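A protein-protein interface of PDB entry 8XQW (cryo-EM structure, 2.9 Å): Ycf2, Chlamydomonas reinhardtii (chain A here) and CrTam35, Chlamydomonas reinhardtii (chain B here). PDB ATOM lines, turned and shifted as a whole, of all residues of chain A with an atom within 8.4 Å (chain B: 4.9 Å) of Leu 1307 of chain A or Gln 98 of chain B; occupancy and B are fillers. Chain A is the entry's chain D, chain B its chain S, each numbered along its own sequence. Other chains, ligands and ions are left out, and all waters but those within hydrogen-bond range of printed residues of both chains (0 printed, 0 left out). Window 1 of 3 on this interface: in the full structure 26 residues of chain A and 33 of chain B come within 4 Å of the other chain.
Of the printed residues of chain B, Lys 1303 of chain A touches Trp 94 and Tyr 95. Printed residues of chain B within 4 Å of Lys 1306 of chain A: Tyr 95 (3.999 Å). Of chain A, only Leu 1307 comes within 4 Å of Gln 98 of chain B.
The side-chain hydroxyl (OG) of Ser 102 of chain B lies close to the side-chain hydroxyl (OG1) of Thr 1311 of chain A, 3.4 Å away.
Hydrophobic or aromatic side chains of chain A that line the printed part of chain B: Leu 1307. Among the printed residues, no Asp or Glu carboxylate lies within 4 Å of a Lys or Arg side-chain nitrogen of the other chain.
O of Gln 98 of chain B is in hydrogen-bond range of OG1 of Thr 101 of chain B (2.7 Å). NE1 of Trp 94 of chain B sits close to NE2 of Gln 98 of chain B (3.0 Å).
Lys 1303 of chain A touches Trp 94 of chain B. CD of Lys 1303 of chain A touches CB of Tyr 95 of chain B (3.9 Å). Tyr 95 of chain B touches Lys 1306 of chain A. Leu 1307 of chain A touches Tyr 95 of chain B (CD2 to CE1, 3.7 Å). Leu 1307 of chain A touches Gln 98 of chain B (CD1 to CB, 3.6 Å).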
ATOM      1  N   MET A 900      41.650  -1.709 -14.646  1.00  0.00           N
ATOM      2  CA  MET A 900      41.851  -0.315 -14.253  1.00  0.00           C
ATOM      3  C   MET A 900      43.342  -0.046 -14.080  1.00  0.00           C
ATOM      4  O   MET A 900      43.971  -0.567 -13.156  1.00  0.00           O
ATOM      5  CB  MET A 900      41.068  -0.007 -12.985  1.00  0.00           C
ATOM      6  CG  MET A 900      39.576  -0.239 -13.146  1.00  0.00           C
ATOM      7  SD  MET A 900      38.677  -0.407 -11.599  1.00  0.00           S
ATOM      8  CE  MET A 900      37.035  -0.784 -12.199  1.00  0.00           C
ATOM      9  N   LEU A1254      15.913   1.415 -15.452  1.00  0.00           N
ATOM     10  CA  LEU A1254      17.162   2.162 -15.445  1.00  0.00           C
ATOM     11  C   LEU A1254      18.157   1.591 -16.443  1.00  0.00           C
ATOM     12  O   LEU A1254      18.984   2.330 -16.985  1.00  0.00           O
ATOM     13  CB  LEU A1254      17.768   2.162 -14.047  1.00  0.00           C
ATOM     14  CG  LEU A1254      17.386   3.337 -13.159  1.00  0.00           C
ATOM     15  CD1 LEU A1254      18.289   3.363 -11.950  1.00  0.00           C
ATOM     16  CD2 LEU A1254      17.468   4.638 -13.928  1.00  0.00           C
ATOM     17  N   TRP A1255      18.098   0.287 -16.694  1.00  0.00           N
ATOM     18  CA  TRP A1255      19.060  -0.369 -17.565  1.00  0.00           C
ATOM     19  C   TRP A1255      18.510  -0.694 -18.941  1.00  0.00           C
ATOM     20  O   TRP A1255      19.291  -0.998 -19.846  1.00  0.00           O
ATOM     21  CB  TRP A1255      19.571  -1.655 -16.916  1.00  0.00           C
ATOM     22  CG  TRP A1255      20.773  -1.434 -16.076  1.00  0.00           C
ATOM     23  CD1 TRP A1255      22.065  -1.451 -16.487  1.00  0.00           C
ATOM     24  CD2 TRP A1255      20.800  -1.153 -14.678  1.00  0.00           C
ATOM     25  NE1 TRP A1255      22.903  -1.202 -15.430  1.00  0.00           N
ATOM     26  CE2 TRP A1255      22.147  -1.014 -14.306  1.00  0.00           C
ATOM     27  CE3 TRP A1255      19.817  -1.007 -13.701  1.00  0.00           C
ATOM     28  CZ2 TRP A1255      22.534  -0.734 -13.002  1.00  0.00           C
ATOM     29  CZ3 TRP A1255      20.204  -0.732 -12.411  1.00  0.00           C
ATOM     30  CH2 TRP A1255      21.550  -0.596 -12.072  1.00  0.00           C
ATOM     31  N   VAL A1300      22.883  12.913 -15.163  1.00  0.00           N
ATOM     32  CA  VAL A1300      23.691  12.566 -13.994  1.00  0.00           C
ATOM     33  C   VAL A1300      22.828  11.967 -12.889  1.00  0.00           C
ATOM     34  O   VAL A1300      23.308  11.142 -12.104  1.00  0.00           O
ATOM     35  CB  VAL A1300      24.502  13.771 -13.486  1.00  0.00           C
ATOM     36  CG1 VAL A1300      25.292  14.390 -14.614  1.00  0.00           C
ATOM     37  CG2 VAL A1300      23.603  14.793 -12.816  1.00  0.00           C
ATOM     38  N   LYS A1301      21.548  12.337 -12.809  1.00  0.00           N
ATOM     39  CA  LYS A1301      20.688  11.719 -11.806  1.00  0.00           C
ATOM     40  C   LYS A1301      20.472  10.246 -12.104  1.00  0.00           C
ATOM     41  O   LYS A1301      20.578   9.403 -11.203  1.00  0.00           O
ATOM     42  CB  LYS A1301      19.349  12.444 -11.726  1.00  0.00           C
ATOM     43  CG  LYS A1301      19.206  13.323 -10.501  1.00  0.00           C
ATOM     44  CD  LYS A1301      20.434  14.194 -10.313  1.00  0.00           C
ATOM     45  CE  LYS A1301      20.187  15.299  -9.303  1.00  0.00           C
ATOM     46  NZ  LYS A1301      21.338  16.243  -9.223  1.00  0.00           N
ATOM     47  N   GLN A1302      20.162   9.916 -13.355  1.00  0.00           N
ATOM     48  CA  GLN A1302      20.030   8.506 -13.700  1.00  0.00           C
ATOM     49  C   GLN A1302      21.324   7.750 -13.421  1.00  0.00           C
ATOM     50  O   GLN A1302      21.297   6.603 -12.954  1.00  0.00           O
ATOM     51  CB  GLN A1302      19.629   8.355 -15.160  1.00  0.00           C
ATOM     52  CG  GLN A1302      18.146   8.415 -15.395  1.00  0.00           C
ATOM     53  CD  GLN A1302      17.821   8.522 -16.860  1.00  0.00           C
ATOM     54  OE1 GLN A1302      18.573   9.120 -17.626  1.00  0.00           O
ATOM     55  NE2 GLN A1302      16.697   7.943 -17.263  1.00  0.00           N
ATOM     56  N   LYS A1303      22.469   8.377 -13.695  1.00  0.00           N
ATOM     57  CA  LYS A1303      23.735   7.701 -13.426  1.00  0.00           C
ATOM     58  C   LYS A1303      23.942   7.465 -11.935  1.00  0.00           C
ATOM     59  O   LYS A1303      24.441   6.405 -11.535  1.00  0.00           O
ATOM     60  CB  LYS A1303      24.891   8.506 -14.008  1.00  0.00           C
ATOM     61  CG  LYS A1303      24.943   8.487 -15.525  1.00  0.00           C
ATOM     62  CD  LYS A1303      24.958   7.066 -16.052  1.00  0.00           C
ATOM     63  CE  LYS A1303      24.237   6.970 -17.382  1.00  0.00           C
ATOM     64  NZ  LYS A1303      24.128   5.562 -17.829  1.00  0.00           N
ATOM     65  N   LYS A1304      23.566   8.438 -11.099  1.00  0.00           N
ATOM     66  CA  LYS A1304      23.649   8.255  -9.654  1.00  0.00           C
ATOM     67  C   LYS A1304      22.773   7.100  -9.196  1.00  0.00           C
ATOM     68  O   LYS A1304      23.195   6.283  -8.368  1.00  0.00           O
ATOM     69  CB  LYS A1304      23.232   9.533  -8.938  1.00  0.00           C
ATOM     70  CG  LYS A1304      24.241  10.640  -9.003  1.00  0.00           C
ATOM     71  CD  LYS A1304      23.784  11.817  -8.175  1.00  0.00           C
ATOM     72  CE  LYS A1304      24.774  12.956  -8.244  1.00  0.00           C
ATOM     73  NZ  LYS A1304      24.297  14.131  -7.468  1.00  0.00           N
ATOM     74  N   GLN A1305      21.544   7.034  -9.702  1.00  0.00           N
ATOM     75  CA  GLN A1305      20.658   5.938  -9.331  1.00  0.00           C
ATOM     76  C   GLN A1305      21.268   4.596  -9.702  1.00  0.00           C
ATOM     77  O   GLN A1305      21.237   3.647  -8.907  1.00  0.00           O
ATOM     78  CB  GLN A1305      19.302   6.109 -10.000  1.00  0.00           C
ATOM     79  CG  GLN A1305      18.646   7.433  -9.720  1.00  0.00           C
ATOM     80  CD  GLN A1305      17.800   7.398  -8.480  1.00  0.00           C
ATOM     81  OE1 GLN A1305      17.339   6.339  -8.064  1.00  0.00           O
ATOM     82  NE2 GLN A1305      17.595   8.554  -7.871  1.00  0.00           N
ATOM     83  N   LYS A1306      21.821   4.496 -10.911  1.00  0.00           N
ATOM     84  CA  LYS A1306      22.517   3.276 -11.304  1.00  0.00           C
ATOM     85  C   LYS A1306      23.601   2.925 -10.298  1.00  0.00           C
ATOM     86  O   LYS A1306      23.651   1.802  -9.780  1.00  0.00           O
ATOM     87  CB  LYS A1306      23.121   3.444 -12.695  1.00  0.00           C
ATOM     88  CG  LYS A1306      22.172   3.147 -13.834  1.00  0.00           C
ATOM     89  CD  LYS A1306      22.926   2.979 -15.134  1.00  0.00           C
ATOM     90  CE  LYS A1306      22.147   2.122 -16.111  1.00  0.00           C
ATOM     91  NZ  LYS A1306      23.038   1.504 -17.133  1.00  0.00           N
ATOM     92  N   LEU A1307      24.478   3.887 -10.002  1.00  0.00           N
ATOM     93  CA  LEU A1307      25.591   3.617  -9.102  1.00  0.00           C
ATOM     94  C   LEU A1307      25.102   3.100  -7.763  1.00  0.00           C
ATOM     95  O   LEU A1307      25.663   2.149  -7.212  1.00  0.00           O
ATOM     96  CB  LEU A1307      26.414   4.880  -8.904  1.00  0.00           C
ATOM     97  CG  LEU A1307      27.238   5.309 -10.102  1.00  0.00           C
ATOM     98  CD1 LEU A1307      27.522   6.783 -10.019  1.00  0.00           C
ATOM     99  CD2 LEU A1307      28.514   4.513 -10.117  1.00  0.00           C
ATOM    100  N   ASN A1308      24.050   3.715  -7.227  1.00  0.00           N
ATOM    101  CA  ASN A1308      23.550   3.312  -5.920  1.00  0.00           C
ATOM    102  C   ASN A1308      22.974   1.909  -5.960  1.00  0.00           C
ATOM    103  O   ASN A1308      23.173   1.128  -5.026  1.00  0.00           O
ATOM    104  CB  ASN A1308      22.499   4.295  -5.437  1.00  0.00           C
ATOM    105  CG  ASN A1308      21.974   3.945  -4.080  1.00  0.00           C
ATOM    106  OD1 ASN A1308      22.618   4.207  -3.070  1.00  0.00           O
ATOM    107  ND2 ASN A1308      20.796   3.350  -4.042  1.00  0.00           N
ATOM    108  N   TYR A1309      22.252   1.569  -7.029  1.00  0.00           N
ATOM    109  CA  TYR A1309      21.770   0.200  -7.162  1.00  0.00           C
ATOM    110  C   TYR A1309      22.920  -0.778  -7.329  1.00  0.00           C
ATOM    111  O   TYR A1309      22.744  -1.978  -7.109  1.00  0.00           O
ATOM    112  CB  TYR A1309      20.829   0.079  -8.351  1.00  0.00           C
ATOM    113  CG  TYR A1309      19.411   0.479  -8.065  1.00  0.00           C
ATOM    114  CD1 TYR A1309      18.722  -0.058  -6.994  1.00  0.00           C
ATOM    115  CD2 TYR A1309      18.756   1.389  -8.873  1.00  0.00           C
ATOM    116  CE1 TYR A1309      17.421   0.306  -6.737  1.00  0.00           C
ATOM    117  CE2 TYR A1309      17.460   1.760  -8.624  1.00  0.00           C
ATOM    118  CZ  TYR A1309      16.796   1.217  -7.556  1.00  0.00           C
ATOM    119  OH  TYR A1309      15.496   1.592  -7.313  1.00  0.00           O
ATOM    120  N   MET A1310      24.093  -0.291  -7.725  1.00  0.00           N
ATOM    121  CA  MET A1310      25.197  -1.172  -8.081  1.00  0.00           C
ATOM    122  C   MET A1310      26.231  -1.354  -6.980  1.00  0.00           C
ATOM    123  O   MET A1310      26.678  -2.482  -6.758  1.00  0.00           O
ATOM    124  CB  MET A1310      25.897  -0.651  -9.341  1.00  0.00           C
ATOM    125  CG  MET A1310      26.791  -1.668 -10.010  1.00  0.00           C
ATOM    126  SD  MET A1310      26.002  -3.273 -10.160  1.00  0.00           S
ATOM    127  CE  MET A1310      24.772  -2.916 -11.402  1.00  0.00           C
ATOM    128  N   THR A1311      26.630  -0.296  -6.284  1.00  0.00           N
ATOM    129  CA  THR A1311      27.694  -0.432  -5.296  1.00  0.00           C
ATOM    130  C   THR A1311      27.594   0.709  -4.288  1.00  0.00           C
ATOM    131  O   THR A1311      26.567   1.388  -4.193  1.00  0.00           O
ATOM    132  CB  THR A1311      29.060  -0.482  -5.992  1.00  0.00           C
ATOM    133  OG1 THR A1311      30.082  -0.727  -5.020  1.00  0.00           O
ATOM    134  CG2 THR A1311      29.336   0.829  -6.699  1.00  0.00           C
ATOM    135  N   SER A1312      28.668   0.917  -3.530  1.00  0.00           N
ATOM    136  CA  SER A1312      28.687   1.839  -2.394  1.00  0.00           C
ATOM    137  C   SER A1312      28.752   3.277  -2.886  1.00  0.00           C
ATOM    138  O   SER A1312      29.825   3.867  -3.003  1.00  0.00           O
ATOM    139  CB  SER A1312      29.866   1.526  -1.485  1.00  0.00           C
ATOM    140  OG  SER A1312      29.653   0.329  -0.761  1.00  0.00           O
ATOM    141  N   TYR A1313      27.592   3.854  -3.163  1.00  0.00           N
ATOM    142  CA  TYR A1313      27.446   5.285  -3.383  1.00  0.00           C
ATOM    143  C   TYR A1313      26.766   5.897  -2.167  1.00  0.00           C
ATOM    144  O   TYR A1313      25.857   5.306  -1.585  1.00  0.00           O
ATOM    145  CB  TYR A1313      26.642   5.570  -4.654  1.00  0.00           C
ATOM    146  CG  TYR A1313      26.893   6.934  -5.239  1.00  0.00           C
ATOM    147  CD1 TYR A1313      28.160   7.313  -5.642  1.00  0.00           C
ATOM    148  CD2 TYR A1313      25.861   7.843  -5.387  1.00  0.00           C
ATOM    149  CE1 TYR A1313      28.391   8.558  -6.172  1.00  0.00           C
ATOM    150  CE2 TYR A1313      26.084   9.092  -5.914  1.00  0.00           C
ATOM    151  CZ  TYR A1313      27.349   9.445  -6.305  1.00  0.00           C
ATOM    152  OH  TYR A1313      27.568  10.695  -6.833  1.00  0.00           O
ATOM    153  N   LEU A1314      27.207   7.099  -1.781  1.00  0.00           N
ATOM    154  CA  LEU A1314      26.971   7.551  -0.413  1.00  0.00           C
ATOM    155  C   LEU A1314      26.074   8.779  -0.282  1.00  0.00           C
ATOM    156  O   LEU A1314      26.108   9.428   0.763  1.00  0.00           O
ATOM    157  CB  LEU A1314      28.300   7.817   0.296  1.00  0.00           C
ATOM    158  CG  LEU A1314      28.717   6.758   1.321  1.00  0.00           C
ATOM    159  CD1 LEU A1314      28.405   5.364   0.827  1.00  0.00           C
ATOM    160  CD2 LEU A1314      30.191   6.880   1.657  1.00  0.00           C
ATOM    161  N   VAL A1316      22.113   9.010  -1.820  1.00  0.00           N
ATOM    162  CA  VAL A1316      20.956   8.839  -2.693  1.00  0.00           C
ATOM    163  C   VAL A1316      19.939   7.977  -1.972  1.00  0.00           C
ATOM    164  O   VAL A1316      20.274   7.220  -1.058  1.00  0.00           O
ATOM    165  CB  VAL A1316      21.304   8.203  -4.060  1.00  0.00           C
ATOM    166  CG1 VAL A1316      21.535   9.259  -5.118  1.00  0.00           C
ATOM    167  CG2 VAL A1316      22.519   7.336  -3.925  1.00  0.00           C
ATOM    168  N   TRP B  94      31.752   9.632 -17.149  1.00  0.00           N
ATOM    169  CA  TRP B  94      31.574   9.921 -15.731  1.00  0.00           C
ATOM    170  C   TRP B  94      31.152   8.678 -14.962  1.00  0.00           C
ATOM    171  O   TRP B  94      31.611   8.441 -13.841  1.00  0.00           O
ATOM    172  CB  TRP B  94      30.542  11.029 -15.556  1.00  0.00           C
ATOM    173  CG  TRP B  94      30.417  11.475 -14.152  1.00  0.00           C
ATOM    174  CD1 TRP B  94      31.291  12.256 -13.465  1.00  0.00           C
ATOM    175  CD2 TRP B  94      29.358  11.164 -13.246  1.00  0.00           C
ATOM    176  NE1 TRP B  94      30.844  12.456 -12.186  1.00  0.00           N
ATOM    177  CE2 TRP B  94      29.656  11.794 -12.027  1.00  0.00           C
ATOM    178  CE3 TRP B  94      28.184  10.417 -13.348  1.00  0.00           C
ATOM    179  CZ2 TRP B  94      28.824  11.700 -10.919  1.00  0.00           C
ATOM    180  CZ3 TRP B  94      27.363  10.324 -12.250  1.00  0.00           C
ATOM    181  CH2 TRP B  94      27.685  10.960 -11.052  1.00  0.00           C
ATOM    182  N   TYR B  95      30.284   7.868 -15.560  1.00  0.00           N
ATOM    183  CA  TYR B  95      29.794   6.660 -14.909  1.00  0.00           C
ATOM    184  C   TYR B  95      30.923   5.676 -14.639  1.00  0.00           C
ATOM    185  O   TYR B  95      31.032   5.128 -13.535  1.00  0.00           O
ATOM    186  CB  TYR B  95      28.715   6.034 -15.787  1.00  0.00           C
ATOM    187  CG  TYR B  95      28.090   4.775 -15.261  1.00  0.00           C
ATOM    188  CD1 TYR B  95      27.815   4.621 -13.917  1.00  0.00           C
ATOM    189  CD2 TYR B  95      27.745   3.748 -16.118  1.00  0.00           C
ATOM    190  CE1 TYR B  95      27.233   3.472 -13.440  1.00  0.00           C
ATOM    191  CE2 TYR B  95      27.161   2.598 -15.650  1.00  0.00           C
ATOM    192  CZ  TYR B  95      26.907   2.467 -14.311  1.00  0.00           C
ATOM    193  OH  TYR B  95      26.326   1.320 -13.837  1.00  0.00           O
ATOM    194  N   ARG B  96      31.787   5.451 -15.626  1.00  0.00           N
ATOM    195  CA  ARG B  96      32.884   4.514 -15.424  1.00  0.00           C
ATOM    196  C   ARG B  96      33.926   5.082 -14.468  1.00  0.00           C
ATOM    197  O   ARG B  96      34.541   4.337 -13.693  1.00  0.00           O
ATOM    198  CB  ARG B  96      33.507   4.140 -16.763  1.00  0.00           C
ATOM    199  CG  ARG B  96      32.612   3.256 -17.611  1.00  0.00           C
ATOM    200  CD  ARG B  96      33.326   2.742 -18.845  1.00  0.00           C
ATOM    201  NE  ARG B  96      34.045   3.801 -19.542  1.00  0.00           N
ATOM    202  CZ  ARG B  96      33.530   4.534 -20.520  1.00  0.00           C
ATOM    203  NH1 ARG B  96      32.288   4.322 -20.926  1.00  0.00           N
ATOM    204  NH2 ARG B  96      34.262   5.474 -21.094  1.00  0.00           N
ATOM    205  N   ARG B  97      34.124   6.402 -14.486  1.00  0.00           N
ATOM    206  CA  ARG B  97      34.988   7.000 -13.476  1.00  0.00           C
ATOM    207  C   ARG B  97      34.441   6.759 -12.081  1.00  0.00           C
ATOM    208  O   ARG B  97      35.201   6.479 -11.148  1.00  0.00           O
ATOM    209  CB  ARG B  97      35.150   8.495 -13.720  1.00  0.00           C
ATOM    210  CG  ARG B  97      36.132   9.134 -12.767  1.00  0.00           C
ATOM    211  CD  ARG B  97      36.451  10.541 -13.187  1.00  0.00           C
ATOM    212  NE  ARG B  97      35.279  11.399 -13.118  1.00  0.00           N
ATOM    213  CZ  ARG B  97      35.091  12.318 -12.181  1.00  0.00           C
ATOM    214  NH1 ARG B  97      36.002  12.494 -11.239  1.00  0.00           N
ATOM    215  NH2 ARG B  97      33.996  13.057 -12.188  1.00  0.00           N
ATOM    216  N   GLN B  98      33.122   6.870 -11.917  1.00  0.00           N
ATOM    217  CA  GLN B  98      32.528   6.639 -10.606  1.00  0.00           C
ATOM    218  C   GLN B  98      32.685   5.189 -10.177  1.00  0.00           C
ATOM    219  O   GLN B  98      32.969   4.914  -9.008  1.00  0.00           O
ATOM    220  CB  GLN B  98      31.059   7.037 -10.613  1.00  0.00           C
ATOM    221  CG  GLN B  98      30.808   8.528 -10.725  1.00  0.00           C
ATOM    222  CD  GLN B  98      31.617   9.342  -9.747  1.00  0.00           C
ATOM    223  OE1 GLN B  98      31.914   8.898  -8.640  1.00  0.00           O
ATOM    224  NE2 GLN B  98      31.965  10.556 -10.143  1.00  0.00           N
ATOM    225  N   LEU B  99      32.490   4.248 -11.100  1.00  0.00           N
ATOM    226  CA  LEU B  99      32.744   2.847 -10.775  1.00  0.00           C
ATOM    227  C   LEU B  99      34.167   2.652 -10.270  1.00  0.00           C
ATOM    228  O   LEU B  99      34.392   1.995  -9.243  1.00  0.00           O
ATOM    229  CB  LEU B  99      32.481   1.964 -11.989  1.00  0.00           C
ATOM    230  CG  LEU B  99      31.024   1.592 -12.234  1.00  0.00           C
ATOM    231  CD1 LEU B  99      30.623   1.888 -13.653  1.00  0.00           C
ATOM    232  CD2 LEU B  99      30.830   0.131 -11.946  1.00  0.00           C
ATOM    233  N   ARG B 100      35.144   3.219 -10.980  1.00  0.00           N
ATOM    234  CA  ARG B 100      36.531   3.067 -10.548  1.00  0.00           C
ATOM    235  C   ARG B 100      36.745   3.664  -9.167  1.00  0.00           C
ATOM    236  O   ARG B 100      37.338   3.028  -8.291  1.00  0.00           O
ATOM    237  CB  ARG B 100      37.484   3.709 -11.547  1.00  0.00           C
ATOM    238  CG  ARG B 100      38.865   3.949 -10.962  1.00  0.00           C
ATOM    239  CD  ARG B 100      39.743   4.732 -11.913  1.00  0.00           C
ATOM    240  NE  ARG B 100      39.402   6.146 -11.928  1.00  0.00           N
ATOM    241  CZ  ARG B 100      39.839   7.019 -11.031  1.00  0.00           C
ATOM    242  NH1 ARG B 100      40.633   6.617 -10.052  1.00  0.00           N
ATOM    243  NH2 ARG B 100      39.484   8.294 -11.112  1.00  0.00           N
ATOM    244  N   THR B 101      36.276   4.897  -8.955  1.00  0.00           N
ATOM    245  CA  THR B 101      36.481   5.546  -7.664  1.00  0.00           C
ATOM    246  C   THR B 101      35.871   4.733  -6.537  1.00  0.00           C
ATOM    247  O   THR B 101      36.501   4.559  -5.490  1.00  0.00           O
ATOM    248  CB  THR B 101      35.887   6.950  -7.660  1.00  0.00           C
ATOM    249  OG1 THR B 101      34.640   6.940  -8.356  1.00  0.00           O
ATOM    250  CG2 THR B 101      36.819   7.927  -8.340  1.00  0.00           C
ATOM    251  N   SER B 102      34.663   4.210  -6.743  1.00  0.00           N
ATOM    252  CA  SER B 102      34.021   3.395  -5.719  1.00  0.00           C
ATOM    253  C   SER B 102      34.837   2.154  -5.397  1.00  0.00           C
ATOM    254  O   SER B 102      35.114   1.872  -4.225  1.00  0.00           O
ATOM    255  CB  SER B 102      32.620   2.997  -6.171  1.00  0.00           C
ATOM    256  OG  SER B 102      32.326   1.673  -5.769  1.00  0.00           O
